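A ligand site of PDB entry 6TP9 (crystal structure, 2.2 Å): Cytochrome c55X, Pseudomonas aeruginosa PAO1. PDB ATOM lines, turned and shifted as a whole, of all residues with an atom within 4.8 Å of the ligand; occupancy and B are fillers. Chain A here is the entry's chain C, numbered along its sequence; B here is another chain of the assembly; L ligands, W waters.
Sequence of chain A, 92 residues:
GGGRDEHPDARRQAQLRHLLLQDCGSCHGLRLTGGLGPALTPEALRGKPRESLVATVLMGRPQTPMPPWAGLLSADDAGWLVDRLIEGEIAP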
ATOM      1  N   LEU A  36     -10.278  -5.422  10.035  1.00  0.00           N
ATOM      2  CA  LEU A  36      -9.994  -3.991   9.936  1.00  0.00           C
ATOM      3  C   LEU A  36      -9.775  -3.399  11.319  1.00  0.00           C
ATOM      4  O   LEU A  36      -8.885  -2.560  11.507  1.00  0.00           O
ATOM      5  CB  LEU A  36     -11.138  -3.281   9.220  1.00  0.00           C
ATOM      6  CG  LEU A  36     -11.027  -1.762   9.106  1.00  0.00           C
ATOM      7  CD1 LEU A  36      -9.895  -1.377   8.155  1.00  0.00           C
ATOM      8  CD2 LEU A  36     -12.341  -1.138   8.663  1.00  0.00           C
ATOM      9  N   GLY A  37     -10.588  -3.810  12.289  1.00  0.00           N
ATOM     10  CA  GLY A  37     -10.421  -3.382  13.655  1.00  0.00           C
ATOM     11  C   GLY A  37      -9.615  -4.378  14.453  1.00  0.00           C
ATOM     12  O   GLY A  37      -9.418  -5.527  14.031  1.00  0.00           O
ATOM     13  N   PRO A  38      -9.136  -3.971  15.620  1.00  0.00           N
ATOM     14  CA  PRO A  38      -8.306  -4.867  16.427  1.00  0.00           C
ATOM     15  C   PRO A  38      -9.092  -6.061  16.947  1.00  0.00           C
ATOM     16  O   PRO A  38     -10.323  -6.088  16.926  1.00  0.00           O
ATOM     17  CB  PRO A  38      -7.818  -3.973  17.572  1.00  0.00           C
ATOM     18  CG  PRO A  38      -8.883  -2.934  17.698  1.00  0.00           C
ATOM     19  CD  PRO A  38      -9.400  -2.691  16.309  1.00  0.00           C
ATOM     20  N   LEU A  40     -10.886  -8.390  19.492  1.00  0.00           N
ATOM     21  CA  LEU A  40     -11.649  -8.221  20.719  1.00  0.00           C
ATOM     22  C   LEU A  40     -11.640  -9.518  21.519  1.00  0.00           C
ATOM     23  O   LEU A  40     -12.654  -9.926  22.096  1.00  0.00           O
ATOM     24  CB  LEU A  40     -13.064  -7.775  20.420  1.00  0.00           C
ATOM     25  CG  LEU A  40     -13.181  -6.506  19.565  1.00  0.00           C
ATOM     26  CD1 LEU A  40     -14.626  -6.083  19.419  1.00  0.00           C
ATOM     27  CD2 LEU A  40     -12.335  -5.389  20.156  1.00  0.00           C
ATOM     28  N   LEU A  45      -7.571  -7.860  25.042  1.00  0.00           N
ATOM     29  CA  LEU A  45      -8.104  -6.857  25.951  1.00  0.00           C
ATOM     30  C   LEU A  45      -7.563  -7.026  27.367  1.00  0.00           C
ATOM     31  O   LEU A  45      -8.100  -6.420  28.299  1.00  0.00           O
ATOM     32  CB  LEU A  45      -9.630  -6.907  25.965  1.00  0.00           C
ATOM     33  CG  LEU A  45     -10.307  -6.757  24.595  1.00  0.00           C
ATOM     34  CD1 LEU A  45     -11.799  -6.997  24.713  1.00  0.00           C
ATOM     35  CD2 LEU A  45     -10.024  -5.382  24.001  1.00  0.00           C
ATOM     36  N   LYS A  48      -6.649  -3.912  30.053  1.00  0.00           N
ATOM     37  CA  LYS A  48      -7.110  -2.594  29.630  1.00  0.00           C
ATOM     38  C   LYS A  48      -8.277  -2.151  30.504  1.00  0.00           C
ATOM     39  O   LYS A  48      -9.215  -2.936  30.728  1.00  0.00           O
ATOM     40  CB  LYS A  48      -7.531  -2.610  28.161  1.00  0.00           C
ATOM     41  CG  LYS A  48      -6.424  -3.071  27.236  1.00  0.00           C
ATOM     42  CD  LYS A  48      -6.843  -3.005  25.772  1.00  0.00           C
ATOM     43  CE  LYS A  48      -5.645  -3.227  24.856  1.00  0.00           C
ATOM     44  NZ  LYS A  48      -5.971  -2.964  23.435  1.00  0.00           N
ATOM     45  N   LEU A  53     -12.880   0.564  27.494  1.00  0.00           N
ATOM     46  CA  LEU A  53     -13.483  -0.156  26.383  1.00  0.00           C
ATOM     47  C   LEU A  53     -14.935   0.228  26.200  1.00  0.00           C
ATOM     48  O   LEU A  53     -15.438   0.289  25.069  1.00  0.00           O
ATOM     49  CB  LEU A  53     -13.349  -1.667  26.622  1.00  0.00           C
ATOM     50  CG  LEU A  53     -11.912  -2.166  26.769  1.00  0.00           C
ATOM     51  CD1 LEU A  53     -11.897  -3.659  27.045  1.00  0.00           C
ATOM     52  CD2 LEU A  53     -11.102  -1.847  25.521  1.00  0.00           C
ATOM     53  N   THR A  56     -14.992   3.565  24.358  1.00  0.00           N
ATOM     54  CA  THR A  56     -14.746   3.430  22.926  1.00  0.00           C
ATOM     55  C   THR A  56     -16.011   2.984  22.193  1.00  0.00           C
ATOM     56  O   THR A  56     -16.255   3.401  21.058  1.00  0.00           O
ATOM     57  CB  THR A  56     -13.611   2.439  22.676  1.00  0.00           C
ATOM     58  OG1 THR A  56     -12.430   2.884  23.354  1.00  0.00           O
ATOM     59  CG2 THR A  56     -13.334   2.314  21.188  1.00  0.00           C
ATOM     60  N   VAL A  57     -16.817   2.137  22.837  1.00  0.00           N
ATOM     61  CA  VAL A  57     -18.030   1.635  22.187  1.00  0.00           C
ATOM     62  C   VAL A  57     -19.075   2.747  22.087  1.00  0.00           C
ATOM     63  O   VAL A  57     -19.727   2.908  21.056  1.00  0.00           O
ATOM     64  CB  VAL A  57     -18.570   0.412  22.949  1.00  0.00           C
ATOM     65  CG1 VAL A  57     -19.942   0.025  22.425  1.00  0.00           C
ATOM     66  CG2 VAL A  57     -17.603  -0.755  22.830  1.00  0.00           C
ATOM     67  N   ARG A  61     -14.090   6.017  17.985  1.00  0.00           N
ATOM     68  CA  ARG A  61     -12.744   6.573  17.894  1.00  0.00           C
ATOM     69  C   ARG A  61     -12.697   7.507  16.685  1.00  0.00           C
ATOM     70  O   ARG A  61     -12.717   7.023  15.541  1.00  0.00           O
ATOM     71  CB  ARG A  61     -11.693   5.462  17.777  1.00  0.00           C
ATOM     72  CG  ARG A  61     -11.437   4.725  19.087  1.00  0.00           C
ATOM     73  CD  ARG A  61     -10.203   5.259  19.820  1.00  0.00           C
ATOM     74  NE  ARG A  61     -10.066   4.709  21.166  1.00  0.00           N
ATOM     75  CZ  ARG A  61      -9.543   3.515  21.450  1.00  0.00           C
ATOM     76  NH1 ARG A  61      -9.118   2.721  20.482  1.00  0.00           N
ATOM     77  NH2 ARG A  61      -9.466   3.116  22.714  1.00  0.00           N
ATOM     78  N   THR A  64     -11.395   7.183  12.655  1.00  0.00           N
ATOM     79  CA  THR A  64     -11.209   5.761  12.401  1.00  0.00           C
ATOM     80  C   THR A  64     -12.560   5.163  11.999  1.00  0.00           C
ATOM     81  O   THR A  64     -13.598   5.803  12.191  1.00  0.00           O
ATOM     82  CB  THR A  64     -10.652   5.030  13.618  1.00  0.00           C
ATOM     83  OG1 THR A  64     -11.664   4.948  14.634  1.00  0.00           O
ATOM     84  CG2 THR A  64      -9.434   5.751  14.178  1.00  0.00           C
ATOM     85  N   PRO A  65     -12.580   3.956  11.437  1.00  0.00           N
ATOM     86  CA  PRO A  65     -13.867   3.343  11.069  1.00  0.00           C
ATOM     87  C   PRO A  65     -14.713   2.916  12.260  1.00  0.00           C
ATOM     88  O   PRO A  65     -15.876   2.536  12.055  1.00  0.00           O
ATOM     89  CB  PRO A  65     -13.464   2.129  10.214  1.00  0.00           C
ATOM     90  CG  PRO A  65     -12.016   2.328   9.881  1.00  0.00           C
ATOM     91  CD  PRO A  65     -11.434   3.147  10.995  1.00  0.00           C
ATOM     92  N   MET A  66     -14.194   2.968  13.473  1.00  0.00           N
ATOM     93  CA  MET A  66     -14.946   2.558  14.657  1.00  0.00           C
ATOM     94  C   MET A  66     -16.025   3.599  14.978  1.00  0.00           C
ATOM     95  O   MET A  66     -15.684   4.683  15.451  1.00  0.00           O
ATOM     96  CB  MET A  66     -14.015   2.390  15.852  1.00  0.00           C
ATOM     97  CG  MET A  66     -14.733   2.072  17.162  1.00  0.00           C
ATOM     98  SD  MET A  66     -15.830   0.647  17.079  1.00  0.00           S
ATOM     99  CE  MET A  66     -16.717   0.828  18.624  1.00  0.00           C
ATOM    100  N   PRO A  67     -17.303   3.304  14.765  1.00  0.00           N
ATOM    101  CA  PRO A  67     -18.325   4.331  14.965  1.00  0.00           C
ATOM    102  C   PRO A  67     -18.724   4.450  16.414  1.00  0.00           C
ATOM    103  O   PRO A  67     -18.328   3.631  17.262  1.00  0.00           O
ATOM    104  CB  PRO A  67     -19.494   3.830  14.099  1.00  0.00           C
ATOM    105  CG  PRO A  67     -19.280   2.343  13.944  1.00  0.00           C
ATOM    106  CD  PRO A  67     -17.900   1.998  14.440  1.00  0.00           C
ATOM    107  N   TRP A  69     -21.557   4.039  19.232  1.00  0.00           N
ATOM    108  CA  TRP A  69     -22.770   3.238  19.370  1.00  0.00           C
ATOM    109  C   TRP A  69     -23.736   3.781  20.416  1.00  0.00           C
ATOM    110  O   TRP A  69     -24.772   3.153  20.670  1.00  0.00           O
ATOM    111  CB  TRP A  69     -22.399   1.787  19.692  1.00  0.00           C
ATOM    112  CG  TRP A  69     -21.643   1.152  18.563  1.00  0.00           C
ATOM    113  CD1 TRP A  69     -20.292   1.161  18.371  1.00  0.00           C
ATOM    114  CD2 TRP A  69     -22.212   0.447  17.455  1.00  0.00           C
ATOM    115  NE1 TRP A  69     -19.986   0.487  17.219  1.00  0.00           N
ATOM    116  CE2 TRP A  69     -21.135   0.039  16.629  1.00  0.00           C
ATOM    117  CE3 TRP A  69     -23.519   0.106  17.073  1.00  0.00           C
ATOM    118  CZ2 TRP A  69     -21.335  -0.688  15.460  1.00  0.00           C
ATOM    119  CZ3 TRP A  69     -23.708  -0.612  15.906  1.00  0.00           C
ATOM    120  CH2 TRP A  69     -22.625  -1.004  15.118  1.00  0.00           C
ATOM    121  N   LEU A  73     -26.929   2.118  21.959  1.00  0.00           N
ATOM    122  CA  LEU A  73     -26.573   1.362  23.143  1.00  0.00           C
ATOM    123  C   LEU A  73     -26.465   2.291  24.346  1.00  0.00           C
ATOM    124  O   LEU A  73     -25.792   3.321  24.290  1.00  0.00           O
ATOM    125  CB  LEU A  73     -25.243   0.638  22.929  1.00  0.00           C
ATOM    126  CG  LEU A  73     -25.167  -0.265  21.700  1.00  0.00           C
ATOM    127  CD1 LEU A  73     -23.790  -0.904  21.629  1.00  0.00           C
ATOM    128  CD2 LEU A  73     -26.253  -1.334  21.733  1.00  0.00           C
ATOM    129  N   LEU A  81     -21.761  -5.949  26.782  1.00  0.00           N
ATOM    130  CA  LEU A  81     -20.926  -6.432  25.687  1.00  0.00           C
ATOM    131  C   LEU A  81     -19.464  -6.528  26.107  1.00  0.00           C
ATOM    132  O   LEU A  81     -18.825  -7.569  25.906  1.00  0.00           O
ATOM    133  CB  LEU A  81     -21.059  -5.502  24.479  1.00  0.00           C
ATOM    134  CG  LEU A  81     -22.350  -5.567  23.664  1.00  0.00           C
ATOM    135  CD1 LEU A  81     -22.363  -4.464  22.612  1.00  0.00           C
ATOM    136  CD2 LEU A  81     -22.511  -6.927  23.002  1.00  0.00           C
ATOM    137  N   LEU A  85     -16.922  -9.660  25.977  1.00  0.00           N
ATOM    138  CA  LEU A  85     -15.642  -9.692  25.279  1.00  0.00           C
ATOM    139  C   LEU A  85     -14.506 -10.052  26.233  1.00  0.00           C
ATOM    140  O   LEU A  85     -13.576 -10.777  25.862  1.00  0.00           O
ATOM    141  CB  LEU A  85     -15.370  -8.344  24.620  1.00  0.00           C
ATOM    142  CG  LEU A  85     -16.433  -7.863  23.629  1.00  0.00           C
ATOM    143  CD1 LEU A  85     -16.148  -6.437  23.222  1.00  0.00           C
ATOM    144  CD2 LEU A  85     -16.477  -8.776  22.425  1.00  0.00           C
ATOM    145  N   LEU B  19     -25.931  -8.431  17.544  1.00  0.00           N
ATOM    146  CA  LEU B  19     -25.183  -7.270  17.075  1.00  0.00           C
ATOM    147  C   LEU B  19     -23.688  -7.541  17.112  1.00  0.00           C
ATOM    148  O   LEU B  19     -22.967  -7.262  16.142  1.00  0.00           O
ATOM    149  CB  LEU B  19     -25.525  -6.050  17.933  1.00  0.00           C
ATOM    150  CG  LEU B  19     -24.784  -4.761  17.590  1.00  0.00           C
ATOM    151  CD1 LEU B  19     -25.306  -4.169  16.292  1.00  0.00           C
ATOM    152  CD2 LEU B  19     -24.916  -3.766  18.736  1.00  0.00           C
ATOM    153  N   LEU B  20     -23.198  -8.096  18.223  1.00  0.00           N
ATOM    154  CA  LEU B  20     -21.766  -8.368  18.340  1.00  0.00           C
ATOM    155  C   LEU B  20     -21.292  -9.294  17.239  1.00  0.00           C
ATOM    156  O   LEU B  20     -20.238  -9.062  16.627  1.00  0.00           O
ATOM    157  CB  LEU B  20     -21.468  -8.975  19.713  1.00  0.00           C
ATOM    158  CG  LEU B  20     -20.004  -9.309  19.989  1.00  0.00           C
ATOM    159  CD1 LEU B  20     -19.160  -8.050  20.021  1.00  0.00           C
ATOM    160  CD2 LEU B  20     -19.871 -10.062  21.311  1.00  0.00           C
ATOM    161  N   ASP B  23     -22.673  -7.623  13.278  1.00  0.00           N
ATOM    162  CA  ASP B  23     -22.273  -6.263  12.926  1.00  0.00           C
ATOM    163  C   ASP B  23     -20.855  -5.955  13.380  1.00  0.00           C
ATOM    164  O   ASP B  23     -19.997  -5.587  12.567  1.00  0.00           O
ATOM    165  CB  ASP B  23     -23.252  -5.244  13.509  1.00  0.00           C
ATOM    166  CG  ASP B  23     -23.086  -3.864  12.902  1.00  0.00           C
ATOM    167  OD1 ASP B  23     -21.927  -3.424  12.735  1.00  0.00           O
ATOM    168  OD2 ASP B  23     -24.113  -3.217  12.594  1.00  0.00           O
ATOM    169  N   CYS B  24     -20.582  -6.088  14.680  1.00  0.00           N
ATOM    170  CA  CYS B  24     -19.239  -5.815  15.185  1.00  0.00           C
ATOM    171  C   CYS B  24     -18.227  -6.800  14.621  1.00  0.00           C
ATOM    172  O   CYS B  24     -17.079  -6.430  14.346  1.00  0.00           O
ATOM    173  CB  CYS B  24     -19.242  -5.887  16.715  1.00  0.00           C
ATOM    174  SG  CYS B  24     -20.611  -5.009  17.514  1.00  0.00           S
ATOM    175  N   SER B  26     -17.810  -8.078  11.748  1.00  0.00           N
ATOM    176  CA  SER B  26     -17.282  -7.820  10.410  1.00  0.00           C
ATOM    177  C   SER B  26     -15.916  -7.155  10.495  1.00  0.00           C
ATOM    178  O   SER B  26     -14.902  -7.694  10.035  1.00  0.00           O
ATOM    179  CB  SER B  26     -18.258  -6.967   9.615  1.00  0.00           C
ATOM    180  OG  SER B  26     -18.364  -5.661  10.165  1.00  0.00           O
ATOM    181  N   CYS B  27     -15.867  -5.954  11.086  1.00  0.00           N
ATOM    182  CA  CYS B  27     -14.603  -5.235  11.198  1.00  0.00           C
ATOM    183  C   CYS B  27     -13.642  -5.946  12.146  1.00  0.00           C
ATOM    184  O   CYS B  27     -12.443  -6.008  11.877  1.00  0.00           O
ATOM    185  CB  CYS B  27     -14.859  -3.811  11.687  1.00  0.00           C
ATOM    186  SG  CYS B  27     -15.724  -2.739  10.521  1.00  0.00           S
ATOM    187  N   HIS B  28     -14.152  -6.471  13.258  1.00  0.00           N
ATOM    188  CA  HIS B  28     -13.319  -7.077  14.278  1.00  0.00           C
ATOM    189  C   HIS B  28     -13.049  -8.563  14.036  1.00  0.00           C
ATOM    190  O   HIS B  28     -12.548  -9.243  14.933  1.00  0.00           O
ATOM    191  CB  HIS B  28     -13.961  -6.873  15.656  1.00  0.00           C
ATOM    192  CG  HIS B  28     -13.902  -5.459  16.150  1.00  0.00           C
ATOM    193  ND1 HIS B  28     -12.777  -4.922  16.746  1.00  0.00           N
ATOM    194  CD2 HIS B  28     -14.818  -4.465  16.123  1.00  0.00           C
ATOM    195  CE1 HIS B  28     -13.012  -3.667  17.077  1.00  0.00           C
ATOM    196  NE2 HIS B  28     -14.245  -3.364  16.705  1.00  0.00           N
HETATM  197 FE1  LIG L   1     -14.760  -1.418  16.877  1.00  0.00          FE
HETATM  198  C1  LIG L   1     -11.795  -0.220  18.122  1.00  0.00           C
HETATM  199  C2  LIG L   1     -15.653  -2.433  20.056  1.00  0.00           C
HETATM  200  C3  LIG L   1     -17.863  -2.335  15.734  1.00  0.00           C
HETATM  201  C4  LIG L   1     -13.678  -1.036  13.678  1.00  0.00           C
HETATM  202  N1  LIG L   1     -13.905  -1.302  18.742  1.00  0.00           N
HETATM  203  C5  LIG L   1     -12.633  -0.846  19.030  1.00  0.00           C
HETATM  204  C6  LIG L   1     -12.346  -1.134  20.421  1.00  0.00           C
HETATM  205  C7  LIG L   1     -13.417  -1.744  20.944  1.00  0.00           C
HETATM  206  C8  LIG L   1     -14.410  -1.865  19.900  1.00  0.00           C
HETATM  207  C9  LIG L   1     -13.586  -2.246  22.399  1.00  0.00           C
HETATM  208  C10 LIG L   1     -11.039  -0.794  21.175  1.00  0.00           C
HETATM  209  C11 LIG L   1     -10.153  -2.036  21.263  1.00  0.00           C
HETATM  210  C12 LIG L   1      -8.932  -1.747  22.099  1.00  0.00           C
HETATM  211  O1  LIG L   1      -8.925  -0.752  22.859  1.00  0.00           O
HETATM  212  O2  LIG L   1      -7.959  -2.540  22.004  1.00  0.00           O
HETATM  213  N2  LIG L   1     -16.428  -2.251  17.723  1.00  0.00           N
HETATM  214  C13 LIG L   1     -16.610  -2.541  19.063  1.00  0.00           C
HETATM  215  C14 LIG L   1     -17.976  -2.980  19.248  1.00  0.00           C
HETATM  216  C15 LIG L   1     -18.586  -2.947  18.062  1.00  0.00           C
HETATM  217  C16 LIG L   1     -17.626  -2.493  17.081  1.00  0.00           C
HETATM  218  C17 LIG L   1     -18.595  -3.414  20.589  1.00  0.00           C
HETATM  219  C18 LIG L   1     -20.041  -3.346  17.759  1.00  0.00           C
HETATM  220  C19 LIG L   1     -21.030  -2.595  18.670  1.00  0.00           C
HETATM  221  N3  LIG L   1     -15.600  -1.706  15.042  1.00  0.00           N
HETATM  222  C20 LIG L   1     -16.929  -1.968  14.793  1.00  0.00           C
HETATM  223  C21 LIG L   1     -17.152  -1.873  13.369  1.00  0.00           C
HETATM  224  C22 LIG L   1     -16.030  -1.408  12.812  1.00  0.00           C
HETATM  225  C23 LIG L   1     -15.009  -1.359  13.841  1.00  0.00           C
HETATM  226  C24 LIG L   1     -18.551  -1.972  12.709  1.00  0.00           C
HETATM  227  C25 LIG L   1     -15.788  -1.117  11.314  1.00  0.00           C
HETATM  228  C26 LIG L   1     -16.889  -0.215  10.721  1.00  0.00           C
HETATM  229  N4  LIG L   1     -13.008  -0.743  16.035  1.00  0.00           N
HETATM  230  C27 LIG L   1     -12.798  -0.648  14.662  1.00  0.00           C
HETATM  231  C28 LIG L   1     -11.494  -0.065  14.428  1.00  0.00           C
HETATM  232  C29 LIG L   1     -10.913   0.187  15.820  1.00  0.00           C
HETATM  233  C30 LIG L   1     -11.911  -0.267  16.754  1.00  0.00           C
HETATM  234  C31 LIG L   1     -10.833   0.240  13.079  1.00  0.00           C
HETATM  235  C32 LIG L   1      -9.531   0.804  16.132  1.00  0.00           C
HETATM  236  C33 LIG L   1      -9.693   2.327  16.201  1.00  0.00           C
HETATM  237  C34 LIG L   1      -8.377   2.963  16.562  1.00  0.00           C
HETATM  238  O3  LIG L   1      -7.347   2.615  15.936  1.00  0.00           O
HETATM  239  O4  LIG L   1      -8.366   3.832  17.473  1.00  0.00           O
HETATM  240  O   HOH W   1      -7.595   2.058  13.244  1.00  0.00           O
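O4 of the ligand is in salt-bridge range of NH1 of Arg 61 (3.3 Å). NE2 of His 28 of chain B binds FE1 of the ligand (2.0 Å). SG of Cys 24 of chain B is covalently linked to C18 of the ligand, 1.8 Å away. An iron atom (FE1) of the ligand is bound by the side-chain sulfur (SD) of Met 66 (2.3 Å). A carbon (C25) of the ligand is bonded to the side-chain sulfur of Cys 27 of chain B. O2 of the ligand is in salt-bridge range of NZ of Lys 48, at 2.5 Å.
The backbone carbonyl oxygen (O) of Cys 27 of chain B lies within hydrogen-bond range of the backbone NH (N) of Gly 37, at 2.9 Å. N of Arg 61 lies within hydrogen-bond range of O of Met 66 (3.3 Å). A ring nitrogen (ND1) of His 28 of chain B lies within hydrogen-bond range of the backbone carbonyl oxygen of Pro 38 (2.7 Å). O of Asp 23 of chain B sits at hydrogen-bond distance from OG of Ser 26 of chain B. N of Trp 69 lies within hydrogen-bond range of O of Val 57. N of Cys 24 of chain B lies within hydrogen-bond range of O of Leu 19 of chain B (3.0 Å). The side-chain hydroxyl (OG1) of Thr 64 lies close to the backbone NH (N) of Met 66, at 3.4 Å. The backbone carbonyl oxygen (O) of Arg 61 is in hydrogen-bond range of the side-chain hydroxyl (OG1) of Thr 64 (2.5 Å).
Residues that only touch the ligand: Pro 65, Pro 38, Trp 69, Gly 37, Leu 53, Val 57, Thr 64, Thr 56, Asp 23 of chain B, Leu 36 and Leu 40. Hydrophobic or aromatic side chains within 4 Å of the ligand: Pro 38, Leu 40, Leu 53, Val 57, Pro 65, Met 66, Trp 69 and His 28 of chain B. Of the 25 residues printed, 17 come within 4 Å of the ligand. The nearest printed residue that does not touch the ligand is Leu 45 (4.04 Å).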
